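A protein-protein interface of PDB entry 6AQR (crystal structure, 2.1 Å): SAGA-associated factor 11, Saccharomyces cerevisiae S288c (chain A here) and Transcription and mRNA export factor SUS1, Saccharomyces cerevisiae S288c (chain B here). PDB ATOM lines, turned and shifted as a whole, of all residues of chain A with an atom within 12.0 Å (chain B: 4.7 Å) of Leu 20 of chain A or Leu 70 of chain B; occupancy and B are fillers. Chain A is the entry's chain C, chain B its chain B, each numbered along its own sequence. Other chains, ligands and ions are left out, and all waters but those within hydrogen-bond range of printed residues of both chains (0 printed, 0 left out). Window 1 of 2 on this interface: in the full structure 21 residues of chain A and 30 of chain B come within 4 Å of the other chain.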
ATOM      1  N   ASP A   9     -14.506  21.695 -22.863  1.00  0.00           N
ATOM      2  CA  ASP A   9     -15.096  20.562 -22.122  1.00  0.00           C
ATOM      3  C   ASP A   9     -15.628  20.873 -20.722  1.00  0.00           C
ATOM      4  O   ASP A   9     -16.660  20.349 -20.342  1.00  0.00           O
ATOM      5  CB  ASP A   9     -14.109  19.406 -21.995  1.00  0.00           C
ATOM      6  CG  ASP A   9     -13.961  18.644 -23.260  1.00  0.00           C
ATOM      7  OD1 ASP A   9     -14.575  19.063 -24.264  1.00  0.00           O
ATOM      8  OD2 ASP A   9     -13.218  17.625 -23.268  1.00  0.00           O
ATOM      9  N   SER A  10     -14.914  21.689 -19.957  1.00  0.00           N
ATOM     10  CA  SER A  10     -15.380  22.146 -18.654  1.00  0.00           C
ATOM     11  C   SER A  10     -16.792  22.741 -18.790  1.00  0.00           C
ATOM     12  O   SER A  10     -17.756  22.230 -18.224  1.00  0.00           O
ATOM     13  CB  SER A  10     -14.399  23.213 -18.099  1.00  0.00           C
ATOM     14  OG  SER A  10     -14.966  24.036 -17.071  1.00  0.00           O
ATOM     15  N   ILE A  11     -16.875  23.842 -19.536  1.00  0.00           N
ATOM     16  CA  ILE A  11     -18.089  24.566 -19.717  1.00  0.00           C
ATOM     17  C   ILE A  11     -19.177  23.703 -20.413  1.00  0.00           C
ATOM     18  O   ILE A  11     -20.296  23.654 -19.921  1.00  0.00           O
ATOM     19  CB  ILE A  11     -17.826  25.959 -20.303  1.00  0.00           C
ATOM     20  CG1 ILE A  11     -17.334  26.832 -19.155  1.00  0.00           C
ATOM     21  CG2 ILE A  11     -19.113  26.548 -20.842  1.00  0.00           C
ATOM     22  CD1 ILE A  11     -16.986  28.236 -19.566  1.00  0.00           C
ATOM     23  N   SER A  12     -18.821  22.963 -21.458  1.00  0.00           N
ATOM     24  CA  SER A  12     -19.775  22.067 -22.080  1.00  0.00           C
ATOM     25  C   SER A  12     -20.447  21.129 -21.068  1.00  0.00           C
ATOM     26  O   SER A  12     -21.664  20.978 -21.114  1.00  0.00           O
ATOM     27  CB  SER A  12     -19.143  21.285 -23.204  1.00  0.00           C
ATOM     28  OG  SER A  12     -18.811  22.196 -24.250  1.00  0.00           O
ATOM     29  N   ASN A  13     -19.667  20.563 -20.141  1.00  0.00           N
ATOM     30  CA  ASN A  13     -20.172  19.604 -19.160  1.00  0.00           C
ATOM     31  C   ASN A  13     -21.054  20.297 -18.207  1.00  0.00           C
ATOM     32  O   ASN A  13     -22.029  19.725 -17.787  1.00  0.00           O
ATOM     33  CB  ASN A  13     -19.049  18.937 -18.319  1.00  0.00           C
ATOM     34  CG  ASN A  13     -18.269  17.908 -19.085  1.00  0.00           C
ATOM     35  OD1 ASN A  13     -18.770  17.258 -20.019  1.00  0.00           O
ATOM     36  ND2 ASN A  13     -17.009  17.734 -18.680  1.00  0.00           N
ATOM     37  N   GLY A  14     -20.665  21.489 -17.794  1.00  0.00           N
ATOM     38  CA  GLY A  14     -21.478  22.285 -16.865  1.00  0.00           C
ATOM     39  C   GLY A  14     -22.857  22.595 -17.479  1.00  0.00           C
ATOM     40  O   GLY A  14     -23.853  22.602 -16.776  1.00  0.00           O
ATOM     41  N   ILE A  15     -22.918  22.824 -18.803  1.00  0.00           N
ATOM     42  CA  ILE A  15     -24.133  23.279 -19.422  1.00  0.00           C
ATOM     43  C   ILE A  15     -25.021  22.044 -19.498  1.00  0.00           C
ATOM     44  O   ILE A  15     -26.196  22.101 -19.133  1.00  0.00           O
ATOM     45  CB  ILE A  15     -23.880  23.905 -20.819  1.00  0.00           C
ATOM     46  CG1 ILE A  15     -23.345  25.324 -20.665  1.00  0.00           C
ATOM     47  CG2 ILE A  15     -25.160  23.839 -21.683  1.00  0.00           C
ATOM     48  CD1 ILE A  15     -22.725  25.828 -21.914  1.00  0.00           C
ATOM     49  N   LEU A  16     -24.453  20.924 -19.920  1.00  0.00           N
ATOM     50  CA  LEU A  16     -25.198  19.712 -19.958  1.00  0.00           C
ATOM     51  C   LEU A  16     -25.721  19.301 -18.552  1.00  0.00           C
ATOM     52  O   LEU A  16     -26.837  18.802 -18.441  1.00  0.00           O
ATOM     53  CB  LEU A  16     -24.384  18.606 -20.577  1.00  0.00           C
ATOM     54  CG  LEU A  16     -24.931  17.193 -20.535  1.00  0.00           C
ATOM     55  CD1 LEU A  16     -26.200  17.053 -21.375  1.00  0.00           C
ATOM     56  CD2 LEU A  16     -23.882  16.187 -20.986  1.00  0.00           C
ATOM     57  N   ASN A  17     -24.949  19.556 -17.490  1.00  0.00           N
ATOM     58  CA  ASN A  17     -25.319  19.070 -16.192  1.00  0.00           C
ATOM     59  C   ASN A  17     -26.455  19.980 -15.687  1.00  0.00           C
ATOM     60  O   ASN A  17     -27.311  19.514 -14.981  1.00  0.00           O
ATOM     61  CB  ASN A  17     -24.097  19.059 -15.254  1.00  0.00           C
ATOM     62  CG  ASN A  17     -24.457  18.712 -13.823  1.00  0.00           C
ATOM     63  OD1 ASN A  17     -24.580  19.587 -12.942  1.00  0.00           O
ATOM     64  ND2 ASN A  17     -24.678  17.444 -13.590  1.00  0.00           N
ATOM     65  N   ASN A  18     -26.453  21.269 -16.053  1.00  0.00           N
ATOM     66  CA  ASN A  18     -27.602  22.142 -15.800  1.00  0.00           C
ATOM     67  C   ASN A  18     -28.918  21.599 -16.454  1.00  0.00           C
ATOM     68  O   ASN A  18     -29.947  21.504 -15.804  1.00  0.00           O
ATOM     69  CB  ASN A  18     -27.280  23.585 -16.251  1.00  0.00           C
ATOM     70  CG  ASN A  18     -26.519  24.377 -15.177  1.00  0.00           C
ATOM     71  OD1 ASN A  18     -25.905  23.823 -14.311  1.00  0.00           O
ATOM     72  ND2 ASN A  18     -26.601  25.670 -15.230  1.00  0.00           N
ATOM     73  N   LEU A  19     -28.854  21.233 -17.736  1.00  0.00           N
ATOM     74  CA  LEU A  19     -29.991  20.665 -18.449  1.00  0.00           C
ATOM     75  C   LEU A  19     -30.455  19.346 -17.852  1.00  0.00           C
ATOM     76  O   LEU A  19     -31.668  19.141 -17.662  1.00  0.00           O
ATOM     77  CB  LEU A  19     -29.632  20.443 -19.933  1.00  0.00           C
ATOM     78  CG  LEU A  19     -29.391  21.764 -20.633  1.00  0.00           C
ATOM     79  CD1 LEU A  19     -28.531  21.398 -21.876  1.00  0.00           C
ATOM     80  CD2 LEU A  19     -30.716  22.423 -20.962  1.00  0.00           C
ATOM     81  N   LEU A  20     -29.510  18.466 -17.533  1.00  0.00           N
ATOM     82  CA  LEU A  20     -29.845  17.114 -17.017  1.00  0.00           C
ATOM     83  C   LEU A  20     -30.481  17.162 -15.642  1.00  0.00           C
ATOM     84  O   LEU A  20     -31.501  16.508 -15.411  1.00  0.00           O
ATOM     85  CB  LEU A  20     -28.646  16.174 -17.004  1.00  0.00           C
ATOM     86  CG  LEU A  20     -28.296  15.621 -18.389  1.00  0.00           C
ATOM     87  CD1 LEU A  20     -26.955  14.844 -18.289  1.00  0.00           C
ATOM     88  CD2 LEU A  20     -29.429  14.741 -18.971  1.00  0.00           C
ATOM     89  N   THR A  21     -29.905  17.959 -14.753  1.00  0.00           N
ATOM     90  CA  THR A  21     -30.414  18.019 -13.371  1.00  0.00           C
ATOM     91  C   THR A  21     -31.771  18.751 -13.326  1.00  0.00           C
ATOM     92  O   THR A  21     -32.595  18.444 -12.492  1.00  0.00           O
ATOM     93  CB  THR A  21     -29.398  18.732 -12.404  1.00  0.00           C
ATOM     94  OG1 THR A  21     -29.022  20.031 -12.945  1.00  0.00           O
ATOM     95  CG2 THR A  21     -28.184  17.843 -12.189  1.00  0.00           C
ATOM     96  N   THR A  22     -31.963  19.763 -14.197  1.00  0.00           N
ATOM     97  CA  THR A  22     -33.224  20.414 -14.349  1.00  0.00           C
ATOM     98  C   THR A  22     -34.303  19.460 -14.754  1.00  0.00           C
ATOM     99  O   THR A  22     -35.400  19.445 -14.142  1.00  0.00           O
ATOM    100  CB  THR A  22     -33.173  21.644 -15.310  1.00  0.00           C
ATOM    101  OG1 THR A  22     -32.326  22.610 -14.700  1.00  0.00           O
ATOM    102  CG2 THR A  22     -34.611  22.307 -15.469  1.00  0.00           C
ATOM    103  N   LEU A  23     -34.016  18.662 -15.769  1.00  0.00           N
ATOM    104  CA  LEU A  23     -34.950  17.717 -16.250  1.00  0.00           C
ATOM    105  C   LEU A  23     -35.204  16.626 -15.199  1.00  0.00           C
ATOM    106  O   LEU A  23     -36.375  16.236 -14.995  1.00  0.00           O
ATOM    107  CB  LEU A  23     -34.434  17.063 -17.517  1.00  0.00           C
ATOM    108  CG  LEU A  23     -35.337  15.967 -18.077  1.00  0.00           C
ATOM    109  CD1 LEU A  23     -36.743  16.471 -18.419  1.00  0.00           C
ATOM    110  CD2 LEU A  23     -34.725  15.368 -19.368  1.00  0.00           C
ATOM    111  N   ILE A  24     -34.158  16.132 -14.548  1.00  0.00           N
ATOM    112  CA  ILE A  24     -34.368  15.094 -13.475  1.00  0.00           C
ATOM    113  C   ILE A  24     -35.310  15.638 -12.380  1.00  0.00           C
ATOM    114  O   ILE A  24     -36.243  14.994 -11.994  1.00  0.00           O
ATOM    115  CB  ILE A  24     -33.032  14.600 -12.852  1.00  0.00           C
ATOM    116  CG1 ILE A  24     -32.281  13.804 -13.910  1.00  0.00           C
ATOM    117  CG2 ILE A  24     -33.270  13.673 -11.626  1.00  0.00           C
ATOM    118  CD1 ILE A  24     -30.847  13.518 -13.605  1.00  0.00           C
ATOM    119  N   GLN A  25     -35.001  16.829 -11.873  1.00  0.00           N
ATOM    120  CA  GLN A  25     -35.778  17.488 -10.825  1.00  0.00           C
ATOM    121  C   GLN A  25     -37.242  17.752 -11.186  1.00  0.00           C
ATOM    122  O   GLN A  25     -38.130  17.712 -10.315  1.00  0.00           O
ATOM    123  CB  GLN A  25     -35.076  18.788 -10.435  1.00  0.00           C
ATOM    124  CG  GLN A  25     -33.822  18.453  -9.654  1.00  0.00           C
ATOM    125  CD  GLN A  25     -32.893  19.651  -9.514  1.00  0.00           C
ATOM    126  OE1 GLN A  25     -33.346  20.745  -9.302  1.00  0.00           O
ATOM    127  NE2 GLN A  25     -31.591  19.443  -9.666  1.00  0.00           N
ATOM    128  N   ASP A  26     -37.489  18.027 -12.475  1.00  0.00           N
ATOM    129  CA  ASP A  26     -38.848  18.166 -12.997  1.00  0.00           C
ATOM    130  C   ASP A  26     -39.592  16.797 -12.948  1.00  0.00           C
ATOM    131  O   ASP A  26     -40.697  16.668 -12.382  1.00  0.00           O
ATOM    132  CB  ASP A  26     -38.793  18.722 -14.444  1.00  0.00           C
ATOM    133  CG  ASP A  26     -40.205  18.866 -15.094  1.00  0.00           C
ATOM    134  OD1 ASP A  26     -40.233  19.001 -16.342  1.00  0.00           O
ATOM    135  OD2 ASP A  26     -41.281  18.898 -14.400  1.00  0.00           O
ATOM    136  N   ILE A  27     -39.002  15.778 -13.567  1.00  0.00           N
ATOM    137  CA  ILE A  27     -39.639  14.453 -13.530  1.00  0.00           C
ATOM    138  C   ILE A  27     -39.896  13.982 -12.073  1.00  0.00           C
ATOM    139  O   ILE A  27     -41.026  13.562 -11.735  1.00  0.00           O
ATOM    140  CB  ILE A  27     -38.771  13.426 -14.223  1.00  0.00           C
ATOM    141  CG1 ILE A  27     -38.674  13.710 -15.735  1.00  0.00           C
ATOM    142  CG2 ILE A  27     -39.333  11.992 -13.924  1.00  0.00           C
ATOM    143  CD1 ILE A  27     -37.437  12.990 -16.348  1.00  0.00           C
ATOM    144  N   VAL A  28     -38.880  14.094 -11.198  1.00  0.00           N
ATOM    145  CA  VAL A  28     -39.022  13.578  -9.822  1.00  0.00           C
ATOM    146  C   VAL A  28     -40.109  14.376  -9.054  1.00  0.00           C
ATOM    147  O   VAL A  28     -40.923  13.788  -8.352  1.00  0.00           O
ATOM    148  CB  VAL A  28     -37.656  13.608  -9.091  1.00  0.00           C
ATOM    149  CG1 VAL A  28     -37.810  13.340  -7.584  1.00  0.00           C
ATOM    150  CG2 VAL A  28     -36.714  12.543  -9.722  1.00  0.00           C
ATOM    151  N   ALA A  29     -40.139  15.706  -9.216  1.00  0.00           N
ATOM    152  CA  ALA A  29     -41.233  16.513  -8.625  1.00  0.00           C
ATOM    153  C   ALA A  29     -42.624  16.084  -9.079  1.00  0.00           C
ATOM    154  O   ALA A  29     -43.564  16.044  -8.291  1.00  0.00           O
ATOM    155  CB  ALA A  29     -41.038  17.975  -8.926  1.00  0.00           C
ATOM    156  N   LEU B  29     -31.498  17.183 -26.713  1.00  0.00           N
ATOM    157  CA  LEU B  29     -31.328  16.379 -25.462  1.00  0.00           C
ATOM    158  C   LEU B  29     -32.624  15.675 -25.079  1.00  0.00           C
ATOM    159  O   LEU B  29     -32.655  14.426 -24.967  1.00  0.00           O
ATOM    160  CB  LEU B  29     -30.751  17.257 -24.296  1.00  0.00           C
ATOM    161  CG  LEU B  29     -30.579  16.535 -22.982  1.00  0.00           C
ATOM    162  CD1 LEU B  29     -29.603  15.383 -23.143  1.00  0.00           C
ATOM    163  CD2 LEU B  29     -30.117  17.482 -21.885  1.00  0.00           C
ATOM    164  N   LEU B  33     -33.359  11.518 -25.094  1.00  0.00           N
ATOM    165  CA  LEU B  33     -33.642  10.856 -23.800  1.00  0.00           C
ATOM    166  C   LEU B  33     -34.967  10.099 -23.845  1.00  0.00           C
ATOM    167  O   LEU B  33     -35.093   8.964 -23.352  1.00  0.00           O
ATOM    168  CB  LEU B  33     -33.650  11.905 -22.688  1.00  0.00           C
ATOM    169  CG  LEU B  33     -32.244  12.432 -22.351  1.00  0.00           C
ATOM    170  CD1 LEU B  33     -32.262  13.556 -21.291  1.00  0.00           C
ATOM    171  CD2 LEU B  33     -31.260  11.324 -21.946  1.00  0.00           C
ATOM    172  N   GLU B  66     -31.310  11.223  -8.210  1.00  0.00           N
ATOM    173  CA  GLU B  66     -30.507  12.073  -9.078  1.00  0.00           C
ATOM    174  C   GLU B  66     -29.140  11.468  -9.553  1.00  0.00           C
ATOM    175  O   GLU B  66     -28.859  11.462 -10.790  1.00  0.00           O
ATOM    176  CB  GLU B  66     -30.387  13.518  -8.534  1.00  0.00           C
ATOM    177  CG  GLU B  66     -29.695  14.430  -9.536  1.00  0.00           C
ATOM    178  CD  GLU B  66     -29.844  15.898  -9.195  1.00  0.00           C
ATOM    179  OE1 GLU B  66     -29.088  16.369  -8.315  1.00  0.00           O
ATOM    180  OE2 GLU B  66     -30.708  16.577  -9.814  1.00  0.00           O
ATOM    181  N   PRO B  67     -28.310  10.947  -8.606  1.00  0.00           N
ATOM    182  CA  PRO B  67     -27.083  10.328  -9.046  1.00  0.00           C
ATOM    183  C   PRO B  67     -27.324   9.102  -9.943  1.00  0.00           C
ATOM    184  O   PRO B  67     -26.638   8.933 -10.932  1.00  0.00           O
ATOM    185  CB  PRO B  67     -26.433   9.926  -7.722  1.00  0.00           C
ATOM    186  CG  PRO B  67     -26.856  10.993  -6.778  1.00  0.00           C
ATOM    187  CD  PRO B  67     -28.304  11.104  -7.125  1.00  0.00           C
ATOM    188  N   LYS B  68     -28.277   8.256  -9.626  1.00  0.00           N
ATOM    189  CA  LYS B  68     -28.562   7.134 -10.542  1.00  0.00           C
ATOM    190  C   LYS B  68     -29.140   7.594 -11.917  1.00  0.00           C
ATOM    191  O   LYS B  68     -28.843   6.991 -12.927  1.00  0.00           O
ATOM    192  CB  LYS B  68     -29.500   6.113  -9.930  1.00  0.00           C
ATOM    193  CG  LYS B  68     -29.131   5.647  -8.521  1.00  0.00           C
ATOM    194  CD  LYS B  68     -29.948   4.427  -8.145  1.00  0.00           C
ATOM    195  CE  LYS B  68     -29.647   3.995  -6.708  1.00  0.00           C
ATOM    196  NZ  LYS B  68     -30.795   3.186  -6.209  1.00  0.00           N
ATOM    197  N   ALA B  69     -29.952   8.659 -11.956  1.00  0.00           N
ATOM    198  CA  ALA B  69     -30.499   9.121 -13.235  1.00  0.00           C
ATOM    199  C   ALA B  69     -29.394   9.669 -14.147  1.00  0.00           C
ATOM    200  O   ALA B  69     -29.444   9.474 -15.350  1.00  0.00           O
ATOM    201  CB  ALA B  69     -31.597  10.148 -13.009  1.00  0.00           C
ATOM    202  N   LEU B  70     -28.437  10.399 -13.575  1.00  0.00           N
ATOM    203  CA  LEU B  70     -27.308  10.918 -14.318  1.00  0.00           C
ATOM    204  C   LEU B  70     -26.471   9.785 -14.940  1.00  0.00           C
ATOM    205  O   LEU B  70     -26.047   9.891 -16.096  1.00  0.00           O
ATOM    206  CB  LEU B  70     -26.434  11.790 -13.439  1.00  0.00           C
ATOM    207  CG  LEU B  70     -26.972  13.165 -13.050  1.00  0.00           C
ATOM    208  CD1 LEU B  70     -26.160  13.830 -11.918  1.00  0.00           C
ATOM    209  CD2 LEU B  70     -27.049  14.063 -14.269  1.00  0.00           C
ATOM    210  N   GLU B  71     -26.282   8.695 -14.197  1.00  0.00           N
ATOM    211  CA  GLU B  71     -25.541   7.508 -14.694  1.00  0.00           C
ATOM    212  C   GLU B  71     -26.280   6.743 -15.754  1.00  0.00           C
ATOM    213  O   GLU B  71     -25.657   6.074 -16.587  1.00  0.00           O
ATOM    214  CB  GLU B  71     -25.161   6.551 -13.531  1.00  0.00           C
ATOM    215  CG  GLU B  71     -23.876   6.939 -12.791  1.00  0.00           C
ATOM    216  CD  GLU B  71     -22.674   6.944 -13.735  1.00  0.00           C
ATOM    217  OE1 GLU B  71     -22.431   5.902 -14.394  1.00  0.00           O
ATOM    218  OE2 GLU B  71     -21.995   7.992 -13.846  1.00  0.00           O
ATOM    219  N   MET B  72     -27.605   6.819 -15.740  1.00  0.00           N
ATOM    220  CA  MET B  72     -28.387   6.117 -16.748  1.00  0.00           C
ATOM    221  C   MET B  72     -28.381   6.737 -18.154  1.00  0.00           C
ATOM    222  O   MET B  72     -28.849   6.069 -19.105  1.00  0.00           O
ATOM    223  CB  MET B  72     -29.828   5.931 -16.295  1.00  0.00           C
ATOM    224  CG  MET B  72     -30.007   4.993 -15.123  1.00  0.00           C
ATOM    225  SD  MET B  72     -31.632   5.301 -14.365  1.00  0.00           S
ATOM    226  CE  MET B  72     -32.781   4.562 -15.470  1.00  0.00           C
ATOM    227  N   VAL B  73     -27.938   8.003 -18.275  1.00  0.00           N
ATOM    228  CA  VAL B  73     -27.801   8.644 -19.576  1.00  0.00           C
ATOM    229  C   VAL B  73     -26.816   7.843 -20.479  1.00  0.00           C
ATOM    230  O   VAL B  73     -25.692   7.660 -20.109  1.00  0.00           O
ATOM    231  CB  VAL B  73     -27.333  10.109 -19.446  1.00  0.00           C
ATOM    232  CG1 VAL B  73     -27.194  10.756 -20.845  1.00  0.00           C
ATOM    233  CG2 VAL B  73     -28.347  10.906 -18.626  1.00  0.00           C
ATOM    234  N   ARG B  78     -24.973  11.405 -24.389  1.00  0.00           N
ATOM    235  CA  ARG B  78     -24.048  12.297 -23.694  1.00  0.00           C
ATOM    236  C   ARG B  78     -22.999  12.878 -24.663  1.00  0.00           C
ATOM    237  O   ARG B  78     -22.730  14.085 -24.651  1.00  0.00           O
ATOM    238  CB  ARG B  78     -23.353  11.541 -22.566  1.00  0.00           C
ATOM    239  CG  ARG B  78     -22.566  12.448 -21.635  1.00  0.00           C
ATOM    240  CD  ARG B  78     -21.967  11.673 -20.484  1.00  0.00           C
ATOM    241  NE  ARG B  78     -22.963  11.420 -19.453  1.00  0.00           N
ATOM    242  CZ  ARG B  78     -23.246  12.288 -18.489  1.00  0.00           C
ATOM    243  NH1 ARG B  78     -22.619  13.480 -18.449  1.00  0.00           N
ATOM    244  NH2 ARG B  78     -24.171  11.978 -17.583  1.00  0.00           N
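The backbone carbonyl oxygen of Leu 70 of chain B is in hydrogen-bond range of the guanidinium group of Arg 78 of chain B, at 3.2 Å.
The backbone carbonyl oxygen (O) of Asn 17 of chain A is in hydrogen-bond range of the side-chain hydroxyl (OG1) of Thr 21 of chain A.
The backbone carbonyl oxygen (O) of Asn 18 of chain A sits at hydrogen-bond distance from the side-chain hydroxyl (OG1) of Thr 21 of chain A (3.3 Å).
O of Thr 21 of chain A lies close to NE2 of Gln 25 of chain A.
OE2 of Glu 66 of chain B sits at hydrogen-bond distance from NE2 of Gln 25 of chain A.
Of the printed residues of chain B, Thr 21 of chain A touches Glu 66.
Thr 22 of chain A touches none of the printed residues of chain B.
Printed residues of chain B within 4 Å of Ile 24 of chain A: Ala 69 (3.5 Å) and Leu 70 (3.9 Å).
Ile 27 of chain A touches none of the printed residues of chain B.
Of chain A, only Ile 24 comes within 4 Å of Ala 69 of chain B.
Leu 70 of chain B touches just these residues of chain A: Leu 20 and Ile 24.
No residue of chain A comes within 4 Å of Glu 71 of chain B.
No residue of chain A comes within 4 Å of Met 72 of chain B.
The nearest printed residue of chain B that does not touch Leu 20 of chain A is Arg 78 of chain B (4.1 Å).
The nearest printed residue of chain B that does not touch Leu 16 of chain A is Leu 70 of chain B (6.3 Å).
Among the printed residues, pairs that only touch across the chains: Leu 16 of chain A with Leu 29 of chain B (3.97 Å), Leu 16 of chain A with Arg 78 of chain B (3.9 Å), Leu 19 of chain A with Leu 29 of chain B (3.6 Å), Leu 20 of chain A with Leu 33 of chain B (3.8 Å), Leu 20 of chain A with Leu 70 of chain B (3.8 Å), Leu 20 of chain A with Val 73 of chain B (3.9996 Å), Thr 21 of chain A with Glu 66 of chain B (3.6 Å), Leu 23 of chain A with Leu 33 of chain B (3.6 Å), Ile 24 of chain A with Ala 69 of chain B (3.5 Å) and Ile 24 of chain A with Leu 70 of chain B (3.9 Å).
Printed residues of chain B that touch a printed residue of chain A: Leu 29, Leu 33, Glu 66, Ala 69, Leu 70, Val 73 and Arg 78.
Hydrophobic or aromatic side chains of chain B within 4 Å of the printed part of chain A: Leu 29, Leu 33, Ala 69, Leu 70 and Val 73.
Of the 21 printed residues of chain A, 7 touch a printed residue of chain B.
Printed residues of chain A that touch a printed residue of chain B: Leu 16, Leu 19, Leu 20, Thr 21, Leu 23, Ile 24 and Gln 25.
Among the printed residues, 11 pairs touch across the chains.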
